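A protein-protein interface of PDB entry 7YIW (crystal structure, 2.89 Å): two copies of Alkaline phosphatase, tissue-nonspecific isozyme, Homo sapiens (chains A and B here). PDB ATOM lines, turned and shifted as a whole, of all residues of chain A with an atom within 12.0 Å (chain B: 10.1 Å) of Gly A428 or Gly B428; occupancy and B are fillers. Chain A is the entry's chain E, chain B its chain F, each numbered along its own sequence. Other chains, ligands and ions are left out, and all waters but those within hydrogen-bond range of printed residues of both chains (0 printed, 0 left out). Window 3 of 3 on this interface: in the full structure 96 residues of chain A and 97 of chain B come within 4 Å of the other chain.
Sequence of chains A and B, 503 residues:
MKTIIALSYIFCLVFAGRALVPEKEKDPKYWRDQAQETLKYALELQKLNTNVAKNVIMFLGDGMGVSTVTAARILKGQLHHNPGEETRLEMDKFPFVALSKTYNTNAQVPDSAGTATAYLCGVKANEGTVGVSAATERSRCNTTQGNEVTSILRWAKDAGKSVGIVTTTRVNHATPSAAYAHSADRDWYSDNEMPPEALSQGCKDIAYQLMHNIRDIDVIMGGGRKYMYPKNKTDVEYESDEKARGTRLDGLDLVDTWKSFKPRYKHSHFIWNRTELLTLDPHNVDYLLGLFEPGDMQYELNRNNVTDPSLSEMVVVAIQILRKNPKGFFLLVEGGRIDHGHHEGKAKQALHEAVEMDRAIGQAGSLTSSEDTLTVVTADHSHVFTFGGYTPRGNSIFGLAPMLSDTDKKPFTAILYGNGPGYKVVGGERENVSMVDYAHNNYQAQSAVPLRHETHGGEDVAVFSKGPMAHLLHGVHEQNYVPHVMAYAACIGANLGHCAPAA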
ATOM      1  N   THR A 407      -8.821  22.654  17.082  1.00  0.00           N
ATOM      2  CA  THR A 407      -8.922  22.584  15.630  1.00  0.00           C
ATOM      3  C   THR A 407     -10.324  22.211  15.154  1.00  0.00           C
ATOM      4  O   THR A 407     -10.876  22.885  14.280  1.00  0.00           O
ATOM      5  CB  THR A 407      -7.896  21.583  15.080  1.00  0.00           C
ATOM      6  OG1 THR A 407      -6.578  22.134  15.207  1.00  0.00           O
ATOM      7  CG2 THR A 407      -8.169  21.274  13.613  1.00  0.00           C
ATOM      8  N   ASP A 408     -10.918  21.152  15.713  1.00  0.00           N
ATOM      9  CA  ASP A 408     -12.255  20.727  15.308  1.00  0.00           C
ATOM     10  C   ASP A 408     -13.266  20.744  16.450  1.00  0.00           C
ATOM     11  O   ASP A 408     -14.351  20.165  16.310  1.00  0.00           O
ATOM     12  CB  ASP A 408     -12.209  19.338  14.658  1.00  0.00           C
ATOM     13  CG  ASP A 408     -11.683  18.251  15.588  1.00  0.00           C
ATOM     14  OD1 ASP A 408     -11.744  18.398  16.828  1.00  0.00           O
ATOM     15  OD2 ASP A 408     -11.205  17.226  15.061  1.00  0.00           O
ATOM     16  N   LYS A 410     -13.937  19.247  19.046  1.00  0.00           N
ATOM     17  CA  LYS A 410     -14.465  18.090  19.750  1.00  0.00           C
ATOM     18  C   LYS A 410     -13.450  17.555  20.756  1.00  0.00           C
ATOM     19  O   LYS A 410     -12.239  17.641  20.530  1.00  0.00           O
ATOM     20  CB  LYS A 410     -14.843  16.986  18.758  1.00  0.00           C
ATOM     21  CG  LYS A 410     -15.784  17.454  17.661  1.00  0.00           C
ATOM     22  CD  LYS A 410     -16.073  16.353  16.659  1.00  0.00           C
ATOM     23  CE  LYS A 410     -14.962  16.248  15.629  1.00  0.00           C
ATOM     24  NZ  LYS A 410     -15.457  16.503  14.247  1.00  0.00           N
ATOM     25  N   TYR A 423      -9.011   4.186  15.374  1.00  0.00           N
ATOM     26  CA  TYR A 423      -9.351   5.140  14.327  1.00  0.00           C
ATOM     27  C   TYR A 423     -10.832   5.035  13.985  1.00  0.00           C
ATOM     28  O   TYR A 423     -11.345   3.945  13.722  1.00  0.00           O
ATOM     29  CB  TYR A 423      -8.479   4.861  13.099  1.00  0.00           C
ATOM     30  CG  TYR A 423      -8.597   5.831  11.937  1.00  0.00           C
ATOM     31  CD1 TYR A 423      -9.775   5.945  11.203  1.00  0.00           C
ATOM     32  CD2 TYR A 423      -7.515   6.613  11.556  1.00  0.00           C
ATOM     33  CE1 TYR A 423      -9.871   6.820  10.138  1.00  0.00           C
ATOM     34  CE2 TYR A 423      -7.602   7.489  10.492  1.00  0.00           C
ATOM     35  CZ  TYR A 423      -8.782   7.588   9.786  1.00  0.00           C
ATOM     36  OH  TYR A 423      -8.874   8.459   8.725  1.00  0.00           O
ATOM     37  N   LYS A 424     -11.522   6.178  13.993  1.00  0.00           N
ATOM     38  CA  LYS A 424     -12.963   6.189  13.733  1.00  0.00           C
ATOM     39  C   LYS A 424     -13.342   7.572  13.199  1.00  0.00           C
ATOM     40  O   LYS A 424     -13.619   8.493  13.969  1.00  0.00           O
ATOM     41  CB  LYS A 424     -13.752   5.840  14.987  1.00  0.00           C
ATOM     42  CG  LYS A 424     -15.246   5.670  14.754  1.00  0.00           C
ATOM     43  CD  LYS A 424     -15.966   5.310  16.043  1.00  0.00           C
ATOM     44  CE  LYS A 424     -17.235   4.518  15.774  1.00  0.00           C
ATOM     45  NZ  LYS A 424     -17.217   3.192  16.452  1.00  0.00           N
ATOM     46  N   VAL A 425     -13.345   7.704  11.874  1.00  0.00           N
ATOM     47  CA  VAL A 425     -13.921   8.866  11.207  1.00  0.00           C
ATOM     48  C   VAL A 425     -15.310   8.478  10.712  1.00  0.00           C
ATOM     49  O   VAL A 425     -15.471   7.510   9.959  1.00  0.00           O
ATOM     50  CB  VAL A 425     -13.014   9.389  10.076  1.00  0.00           C
ATOM     51  CG1 VAL A 425     -11.636   9.744  10.627  1.00  0.00           C
ATOM     52  CG2 VAL A 425     -12.866   8.376   8.938  1.00  0.00           C
ATOM     53  N   VAL A 426     -16.326   9.199  11.180  1.00  0.00           N
ATOM     54  CA  VAL A 426     -17.705   8.850  10.868  1.00  0.00           C
ATOM     55  C   VAL A 426     -18.095   9.461   9.528  1.00  0.00           C
ATOM     56  O   VAL A 426     -18.768  10.497   9.470  1.00  0.00           O
ATOM     57  CB  VAL A 426     -18.663   9.280  12.000  1.00  0.00           C
ATOM     58  CG1 VAL A 426     -18.522   8.341  13.193  1.00  0.00           C
ATOM     59  CG2 VAL A 426     -18.381  10.713  12.444  1.00  0.00           C
ATOM     60  N   GLY A 427     -17.682   8.811   8.444  1.00  0.00           N
ATOM     61  CA  GLY A 427     -17.983   9.298   7.108  1.00  0.00           C
ATOM     62  C   GLY A 427     -17.529  10.720   6.854  1.00  0.00           C
ATOM     63  O   GLY A 427     -18.241  11.487   6.195  1.00  0.00           O
ATOM     64  N   GLY A 428     -16.357  11.089   7.363  1.00  0.00           N
ATOM     65  CA  GLY A 428     -15.856  12.438   7.204  1.00  0.00           C
ATOM     66  C   GLY A 428     -15.059  12.921   8.397  1.00  0.00           C
ATOM     67  O   GLY A 428     -13.825  12.947   8.360  1.00  0.00           O
ATOM     68  N   GLU A 429     -15.754  13.301   9.464  1.00  0.00           N
ATOM     69  CA  GLU A 429     -15.120  13.824  10.662  1.00  0.00           C
ATOM     70  C   GLU A 429     -14.828  12.704  11.656  1.00  0.00           C
ATOM     71  O   GLU A 429     -15.393  11.612  11.583  1.00  0.00           O
ATOM     72  CB  GLU A 429     -16.008  14.877  11.324  1.00  0.00           C
ATOM     73  CG  GLU A 429     -16.007  16.226  10.633  1.00  0.00           C
ATOM     74  CD  GLU A 429     -17.374  16.883  10.653  1.00  0.00           C
ATOM     75  OE1 GLU A 429     -17.886  17.152  11.760  1.00  0.00           O
ATOM     76  OE2 GLU A 429     -17.937  17.125   9.564  1.00  0.00           O
ATOM     77  N   ARG A 430     -13.935  12.995  12.596  1.00  0.00           N
ATOM     78  CA  ARG A 430     -13.646  12.055  13.665  1.00  0.00           C
ATOM     79  C   ARG A 430     -14.711  12.151  14.755  1.00  0.00           C
ATOM     80  O   ARG A 430     -15.422  13.152  14.883  1.00  0.00           O
ATOM     81  CB  ARG A 430     -12.247  12.303  14.232  1.00  0.00           C
ATOM     82  CG  ARG A 430     -12.158  13.409  15.263  1.00  0.00           C
ATOM     83  CD  ARG A 430     -10.778  13.432  15.904  1.00  0.00           C
ATOM     84  NE  ARG A 430     -10.851  13.445  17.359  1.00  0.00           N
ATOM     85  CZ  ARG A 430     -11.074  14.528  18.092  1.00  0.00           C
ATOM     86  NH1 ARG A 430     -11.243  15.717  17.537  1.00  0.00           N
ATOM     87  NH2 ARG A 430     -11.127  14.415  19.417  1.00  0.00           N
ATOM     88  N   GLU A 431     -14.809  11.090  15.551  1.00  0.00           N
ATOM     89  CA  GLU A 431     -15.973  10.888  16.405  1.00  0.00           C
ATOM     90  C   GLU A 431     -15.985  11.855  17.587  1.00  0.00           C
ATOM     91  O   GLU A 431     -14.991  11.991  18.308  1.00  0.00           O
ATOM     92  CB  GLU A 431     -16.001   9.443  16.903  1.00  0.00           C
ATOM     93  CG  GLU A 431     -17.250   9.068  17.678  1.00  0.00           C
ATOM     94  CD  GLU A 431     -17.173   7.669  18.253  1.00  0.00           C
ATOM     95  OE1 GLU A 431     -16.210   7.384  18.997  1.00  0.00           O
ATOM     96  OE2 GLU A 431     -18.073   6.853  17.963  1.00  0.00           O
ATOM     97  N   ASN A 432     -17.121  12.528  17.776  1.00  0.00           N
ATOM     98  CA  ASN A 432     -17.403  13.332  18.965  1.00  0.00           C
ATOM     99  C   ASN A 432     -17.590  12.370  20.134  1.00  0.00           C
ATOM    100  O   ASN A 432     -18.648  11.757  20.288  1.00  0.00           O
ATOM    101  CB  ASN A 432     -18.639  14.200  18.716  1.00  0.00           C
ATOM    102  CG  ASN A 432     -19.088  15.010  19.942  1.00  0.00           C
ATOM    103  OD1 ASN A 432     -18.565  14.856  21.046  1.00  0.00           O
ATOM    104  ND2 ASN A 432     -20.080  15.888  19.732  1.00  0.00           N
ATOM    105  N   GLN A 446      -8.830   6.505  20.262  1.00  0.00           N
ATOM    106  CA  GLN A 446      -8.576   6.888  18.881  1.00  0.00           C
ATOM    107  C   GLN A 446      -7.096   6.762  18.531  1.00  0.00           C
ATOM    108  O   GLN A 446      -6.215   6.908  19.383  1.00  0.00           O
ATOM    109  CB  GLN A 446      -9.056   8.319  18.633  1.00  0.00           C
ATOM    110  CG  GLN A 446     -10.470   8.407  18.083  1.00  0.00           C
ATOM    111  CD  GLN A 446     -11.182   9.679  18.503  1.00  0.00           C
ATOM    112  OE1 GLN A 446     -10.553  10.712  18.727  1.00  0.00           O
ATOM    113  NE2 GLN A 446     -12.504   9.607  18.609  1.00  0.00           N
ATOM    114  N   SER A 447      -6.833   6.489  17.255  1.00  0.00           N
ATOM    115  CA  SER A 447      -5.487   6.291  16.739  1.00  0.00           C
ATOM    116  C   SER A 447      -5.278   7.167  15.511  1.00  0.00           C
ATOM    117  O   SER A 447      -6.214   7.771  14.980  1.00  0.00           O
ATOM    118  CB  SER A 447      -5.233   4.820  16.389  1.00  0.00           C
ATOM    119  OG  SER A 447      -5.378   4.601  14.996  1.00  0.00           O
ATOM    120  N   ALA A 448      -4.023   7.238  15.064  1.00  0.00           N
ATOM    121  CA  ALA A 448      -3.652   8.065  13.921  1.00  0.00           C
ATOM    122  C   ALA A 448      -3.800   7.328  12.597  1.00  0.00           C
ATOM    123  O   ALA A 448      -4.186   7.934  11.591  1.00  0.00           O
ATOM    124  CB  ALA A 448      -2.213   8.562  14.072  1.00  0.00           C
ATOM    125  N   VAL A 449      -3.491   6.036  12.576  1.00  0.00           N
ATOM    126  CA  VAL A 449      -3.578   5.223  11.367  1.00  0.00           C
ATOM    127  C   VAL A 449      -4.468   4.021  11.662  1.00  0.00           C
ATOM    128  O   VAL A 449      -4.261   3.334  12.673  1.00  0.00           O
ATOM    129  CB  VAL A 449      -2.183   4.789  10.888  1.00  0.00           C
ATOM    130  CG1 VAL A 449      -2.291   3.835   9.709  1.00  0.00           C
ATOM    131  CG2 VAL A 449      -1.346   6.008  10.521  1.00  0.00           C
ATOM    132  N   PRO A 450      -5.464   3.729  10.825  1.00  0.00           N
ATOM    133  CA  PRO A 450      -6.355   2.595  11.108  1.00  0.00           C
ATOM    134  C   PRO A 450      -5.699   1.274  10.730  1.00  0.00           C
ATOM    135  O   PRO A 450      -5.188   1.111   9.619  1.00  0.00           O
ATOM    136  CB  PRO A 450      -7.583   2.880  10.237  1.00  0.00           C
ATOM    137  CG  PRO A 450      -7.071   3.711   9.110  1.00  0.00           C
ATOM    138  CD  PRO A 450      -5.793   4.389   9.549  1.00  0.00           C
ATOM    139  N   ASP B 408      -7.213   0.702   5.286  1.00  0.00           N
ATOM    140  CA  ASP B 408      -7.460   1.678   4.227  1.00  0.00           C
ATOM    141  C   ASP B 408      -6.423   1.617   3.108  1.00  0.00           C
ATOM    142  O   ASP B 408      -6.327   2.558   2.311  1.00  0.00           O
ATOM    143  CB  ASP B 408      -7.561   3.100   4.802  1.00  0.00           C
ATOM    144  CG  ASP B 408      -6.255   3.610   5.417  1.00  0.00           C
ATOM    145  OD1 ASP B 408      -5.151   3.169   5.032  1.00  0.00           O
ATOM    146  OD2 ASP B 408      -6.343   4.485   6.303  1.00  0.00           O
ATOM    147  N   LYS B 410      -3.433   2.173   2.584  1.00  0.00           N
ATOM    148  CA  LYS B 410      -2.505   3.274   2.386  1.00  0.00           C
ATOM    149  C   LYS B 410      -1.275   3.096   3.265  1.00  0.00           C
ATOM    150  O   LYS B 410      -1.357   2.495   4.341  1.00  0.00           O
ATOM    151  CB  LYS B 410      -3.164   4.622   2.701  1.00  0.00           C
ATOM    152  CG  LYS B 410      -4.211   5.038   1.694  1.00  0.00           C
ATOM    153  CD  LYS B 410      -4.744   6.419   1.989  1.00  0.00           C
ATOM    154  CE  LYS B 410      -6.189   6.345   2.429  1.00  0.00           C
ATOM    155  NZ  LYS B 410      -6.909   7.587   2.064  1.00  0.00           N
ATOM    156  N   TYR B 423      -2.222  15.657  12.033  1.00  0.00           N
ATOM    157  CA  TYR B 423      -3.520  15.176  11.580  1.00  0.00           C
ATOM    158  C   TYR B 423      -3.892  15.833  10.258  1.00  0.00           C
ATOM    159  O   TYR B 423      -4.110  17.047  10.203  1.00  0.00           O
ATOM    160  CB  TYR B 423      -4.590  15.460  12.639  1.00  0.00           C
ATOM    161  CG  TYR B 423      -5.944  14.844  12.346  1.00  0.00           C
ATOM    162  CD1 TYR B 423      -6.848  15.473  11.496  1.00  0.00           C
ATOM    163  CD2 TYR B 423      -6.322  13.639  12.925  1.00  0.00           C
ATOM    164  CE1 TYR B 423      -8.084  14.916  11.224  1.00  0.00           C
ATOM    165  CE2 TYR B 423      -7.557  13.075  12.660  1.00  0.00           C
ATOM    166  CZ  TYR B 423      -8.434  13.718  11.810  1.00  0.00           C
ATOM    167  OH  TYR B 423      -9.662  13.158  11.547  1.00  0.00           O
ATOM    168  N   LYS B 424      -3.958  15.043   9.189  1.00  0.00           N
ATOM    169  CA  LYS B 424      -4.350  15.535   7.876  1.00  0.00           C
ATOM    170  C   LYS B 424      -5.385  14.592   7.287  1.00  0.00           C
ATOM    171  O   LYS B 424      -5.216  13.369   7.331  1.00  0.00           O
ATOM    172  CB  LYS B 424      -3.147  15.657   6.937  1.00  0.00           C
ATOM    173  CG  LYS B 424      -3.392  16.570   5.753  1.00  0.00           C
ATOM    174  CD  LYS B 424      -2.105  16.863   5.005  1.00  0.00           C
ATOM    175  CE  LYS B 424      -2.165  18.218   4.319  1.00  0.00           C
ATOM    176  NZ  LYS B 424      -0.923  18.506   3.551  1.00  0.00           N
ATOM    177  N   VAL B 425      -6.458  15.165   6.749  1.00  0.00           N
ATOM    178  CA  VAL B 425      -7.559  14.399   6.178  1.00  0.00           C
ATOM    179  C   VAL B 425      -8.096  15.182   4.988  1.00  0.00           C
ATOM    180  O   VAL B 425      -8.589  16.305   5.151  1.00  0.00           O
ATOM    181  CB  VAL B 425      -8.682  14.133   7.199  1.00  0.00           C
ATOM    182  CG1 VAL B 425     -10.007  13.909   6.497  1.00  0.00           C
ATOM    183  CG2 VAL B 425      -8.347  12.935   8.073  1.00  0.00           C
ATOM    184  N   VAL B 426      -7.978  14.607   3.792  1.00  0.00           N
ATOM    185  CA  VAL B 426      -8.489  15.234   2.577  1.00  0.00           C
ATOM    186  C   VAL B 426      -9.953  14.844   2.419  1.00  0.00           C
ATOM    187  O   VAL B 426     -10.311  14.065   1.528  1.00  0.00           O
ATOM    188  CB  VAL B 426      -7.658  14.835   1.341  1.00  0.00           C
ATOM    189  CG1 VAL B 426      -8.034  15.688   0.139  1.00  0.00           C
ATOM    190  CG2 VAL B 426      -6.163  14.952   1.631  1.00  0.00           C
ATOM    191  N   GLY B 427     -10.806  15.369   3.300  1.00  0.00           N
ATOM    192  CA  GLY B 427     -12.232  15.096   3.262  1.00  0.00           C
ATOM    193  C   GLY B 427     -12.573  13.643   3.547  1.00  0.00           C
ATOM    194  O   GLY B 427     -12.700  12.837   2.619  1.00  0.00           O
ATOM    195  N   GLY B 428     -12.708  13.292   4.831  1.00  0.00           N
ATOM    196  CA  GLY B 428     -12.903  11.920   5.265  1.00  0.00           C
ATOM    197  C   GLY B 428     -11.828  10.928   4.872  1.00  0.00           C
ATOM    198  O   GLY B 428     -11.906   9.766   5.283  1.00  0.00           O
ATOM    199  N   GLU B 429     -10.837  11.341   4.082  1.00  0.00           N
ATOM    200  CA  GLU B 429      -9.815  10.451   3.544  1.00  0.00           C
ATOM    201  C   GLU B 429      -8.473  10.811   4.170  1.00  0.00           C
ATOM    202  O   GLU B 429      -7.986  11.932   3.991  1.00  0.00           O
ATOM    203  CB  GLU B 429      -9.757  10.571   2.017  1.00  0.00           C
ATOM    204  CG  GLU B 429      -9.373   9.300   1.267  1.00  0.00           C
ATOM    205  CD  GLU B 429     -10.067   8.076   1.813  1.00  0.00           C
ATOM    206  OE1 GLU B 429     -11.311   7.997   1.715  1.00  0.00           O
ATOM    207  OE2 GLU B 429      -9.364   7.198   2.353  1.00  0.00           O
ATOM    208  N   ARG B 430      -7.884   9.870   4.905  1.00  0.00           N
ATOM    209  CA  ARG B 430      -6.585  10.112   5.524  1.00  0.00           C
ATOM    210  C   ARG B 430      -5.497  10.133   4.453  1.00  0.00           C
ATOM    211  O   ARG B 430      -5.552   9.380   3.479  1.00  0.00           O
ATOM    212  CB  ARG B 430      -6.301   9.049   6.588  1.00  0.00           C
ATOM    213  CG  ARG B 430      -4.841   8.793   6.877  1.00  0.00           C
ATOM    214  CD  ARG B 430      -4.650   7.429   7.507  1.00  0.00           C
ATOM    215  NE  ARG B 430      -3.263   6.994   7.425  1.00  0.00           N
ATOM    216  CZ  ARG B 430      -2.846   5.969   6.695  1.00  0.00           C
ATOM    217  NH1 ARG B 430      -3.689   5.238   5.986  1.00  0.00           N
ATOM    218  NH2 ARG B 430      -1.549   5.674   6.673  1.00  0.00           N
ATOM    219  N   GLU B 431      -4.510  11.011   4.634  1.00  0.00           N
ATOM    220  CA  GLU B 431      -3.596  11.371   3.553  1.00  0.00           C
ATOM    221  C   GLU B 431      -2.739  10.188   3.113  1.00  0.00           C
ATOM    222  O   GLU B 431      -2.014   9.595   3.920  1.00  0.00           O
ATOM    223  CB  GLU B 431      -2.708  12.534   3.986  1.00  0.00           C
ATOM    224  CG  GLU B 431      -2.057  13.264   2.824  1.00  0.00           C
ATOM    225  CD  GLU B 431      -0.940  14.187   3.264  1.00  0.00           C
ATOM    226  OE1 GLU B 431      -0.197  13.821   4.199  1.00  0.00           O
ATOM    227  OE2 GLU B 431      -0.808  15.281   2.676  1.00  0.00           O
ATOM    228  N   ASN B 432      -2.823   9.857   1.823  1.00  0.00           N
ATOM    229  CA  ASN B 432      -1.901   8.943   1.158  1.00  0.00           C
ATOM    230  C   ASN B 432      -0.495   9.531   1.217  1.00  0.00           C
ATOM    231  O   ASN B 432      -0.190  10.492   0.503  1.00  0.00           O
ATOM    232  CB  ASN B 432      -2.366   8.713  -0.287  1.00  0.00           C
ATOM    233  CG  ASN B 432      -1.512   7.706  -1.054  1.00  0.00           C
ATOM    234  OD1 ASN B 432      -0.436   7.301  -0.612  1.00  0.00           O
ATOM    235  ND2 ASN B 432      -2.005   7.304  -2.227  1.00  0.00           N
ATOM    236  N   PRO B 450      -6.468  16.284  15.998  1.00  0.00           N
ATOM    237  CA  PRO B 450      -5.811  17.499  15.506  1.00  0.00           C
ATOM    238  C   PRO B 450      -5.769  18.596  16.557  1.00  0.00           C
ATOM    239  O   PRO B 450      -6.753  18.865  17.252  1.00  0.00           O
ATOM    240  CB  PRO B 450      -6.683  17.908  14.314  1.00  0.00           C
ATOM    241  CG  PRO B 450      -8.041  17.414  14.677  1.00  0.00           C
ATOM    242  CD  PRO B 450      -7.826  16.128  15.445  1.00  0.00           C
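OD1 of Asp B408 is in salt-bridge range of NH1 of Arg B430, 2.7 Å away.
NZ of Lys B410 lies within hydrogen-bond range of O of Arg B430 (2.7 Å).
N of Lys A410 sits close to OD1 of Asp A408.
The guanidinium group (NH1) of Arg A430 is in salt-bridge range of the side-chain carboxylate (OD1) of Asp A408, 2.8 Å away.
The side-chain amide oxygen (OE1) of Gln A446 sits at hydrogen-bond distance from the guanidinium group (NE) of Arg A430 (3.1 Å).
O of Val A449 sits at hydrogen-bond distance from OG of Ser A447, at 2.9 Å.
Among the printed residues, merely in contact across the chains: Pro A450 with Asp B408, Asp A408 with Pro B450, Gly A428 with Gly B428, Tyr A423 with Arg B430, Val A449 with Arg B430, Thr A407 with Pro B450, Arg A430 with Tyr B423 and Pro A450 with Arg B430.
Asp A408 touches Pro B450, and with the chains exchanged Pro A450 touches Asp B408.
Tyr A423 touches Arg B430, and with the chains exchanged Arg A430 touches Tyr B423.
Gly A428 touches its own counterpart, Gly B428.
Pro A450 touches Arg B430, but with the chains exchanged Arg A430 does not touch Pro B450 (4.02 Å).
13 positions are printed for both chains.
Of the 8 pairs that touch across the chains among the printed residues, 5 have their exchanged pair printed and touching as well.
Hydrophobic or aromatic side chains of chain B that line the printed part of chain A: Tyr B423 and Pro B450.
Along chain B the printed residues that touch a printed residue of chain A span positions 408 to 450.
Among the printed residues, 8 pairs touch across the chains.
Among the printed residues, no Asp or Glu carboxylate lies within 4 Å of a Lys or Arg side-chain nitrogen of the other chain.
Of the printed residues of chain B, Asp A408 touches Pro B450 (3.2 Å).
Lys A424 touches none of the printed residues of chain B.
No residue of chain B comes within 4 Å of Gly A427.
Gly A428 touches just one residue of chain B: Gly B428 (3.4 Å).
Of the printed residues of chain B, Arg A430 touches Tyr B423 (3.8 Å).
No residue of chain A comes within 4 Å of Val B426.
No residue of chain A comes within 4 Å of Gly B427.
Gly B428 touches just one residue of chain A: Gly A428 (3.4 Å).
No residue of chain A comes within 4 Å of Glu B429.
Of the printed residues of chain A, Pro B450 touches Thr A407 and Asp A408.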
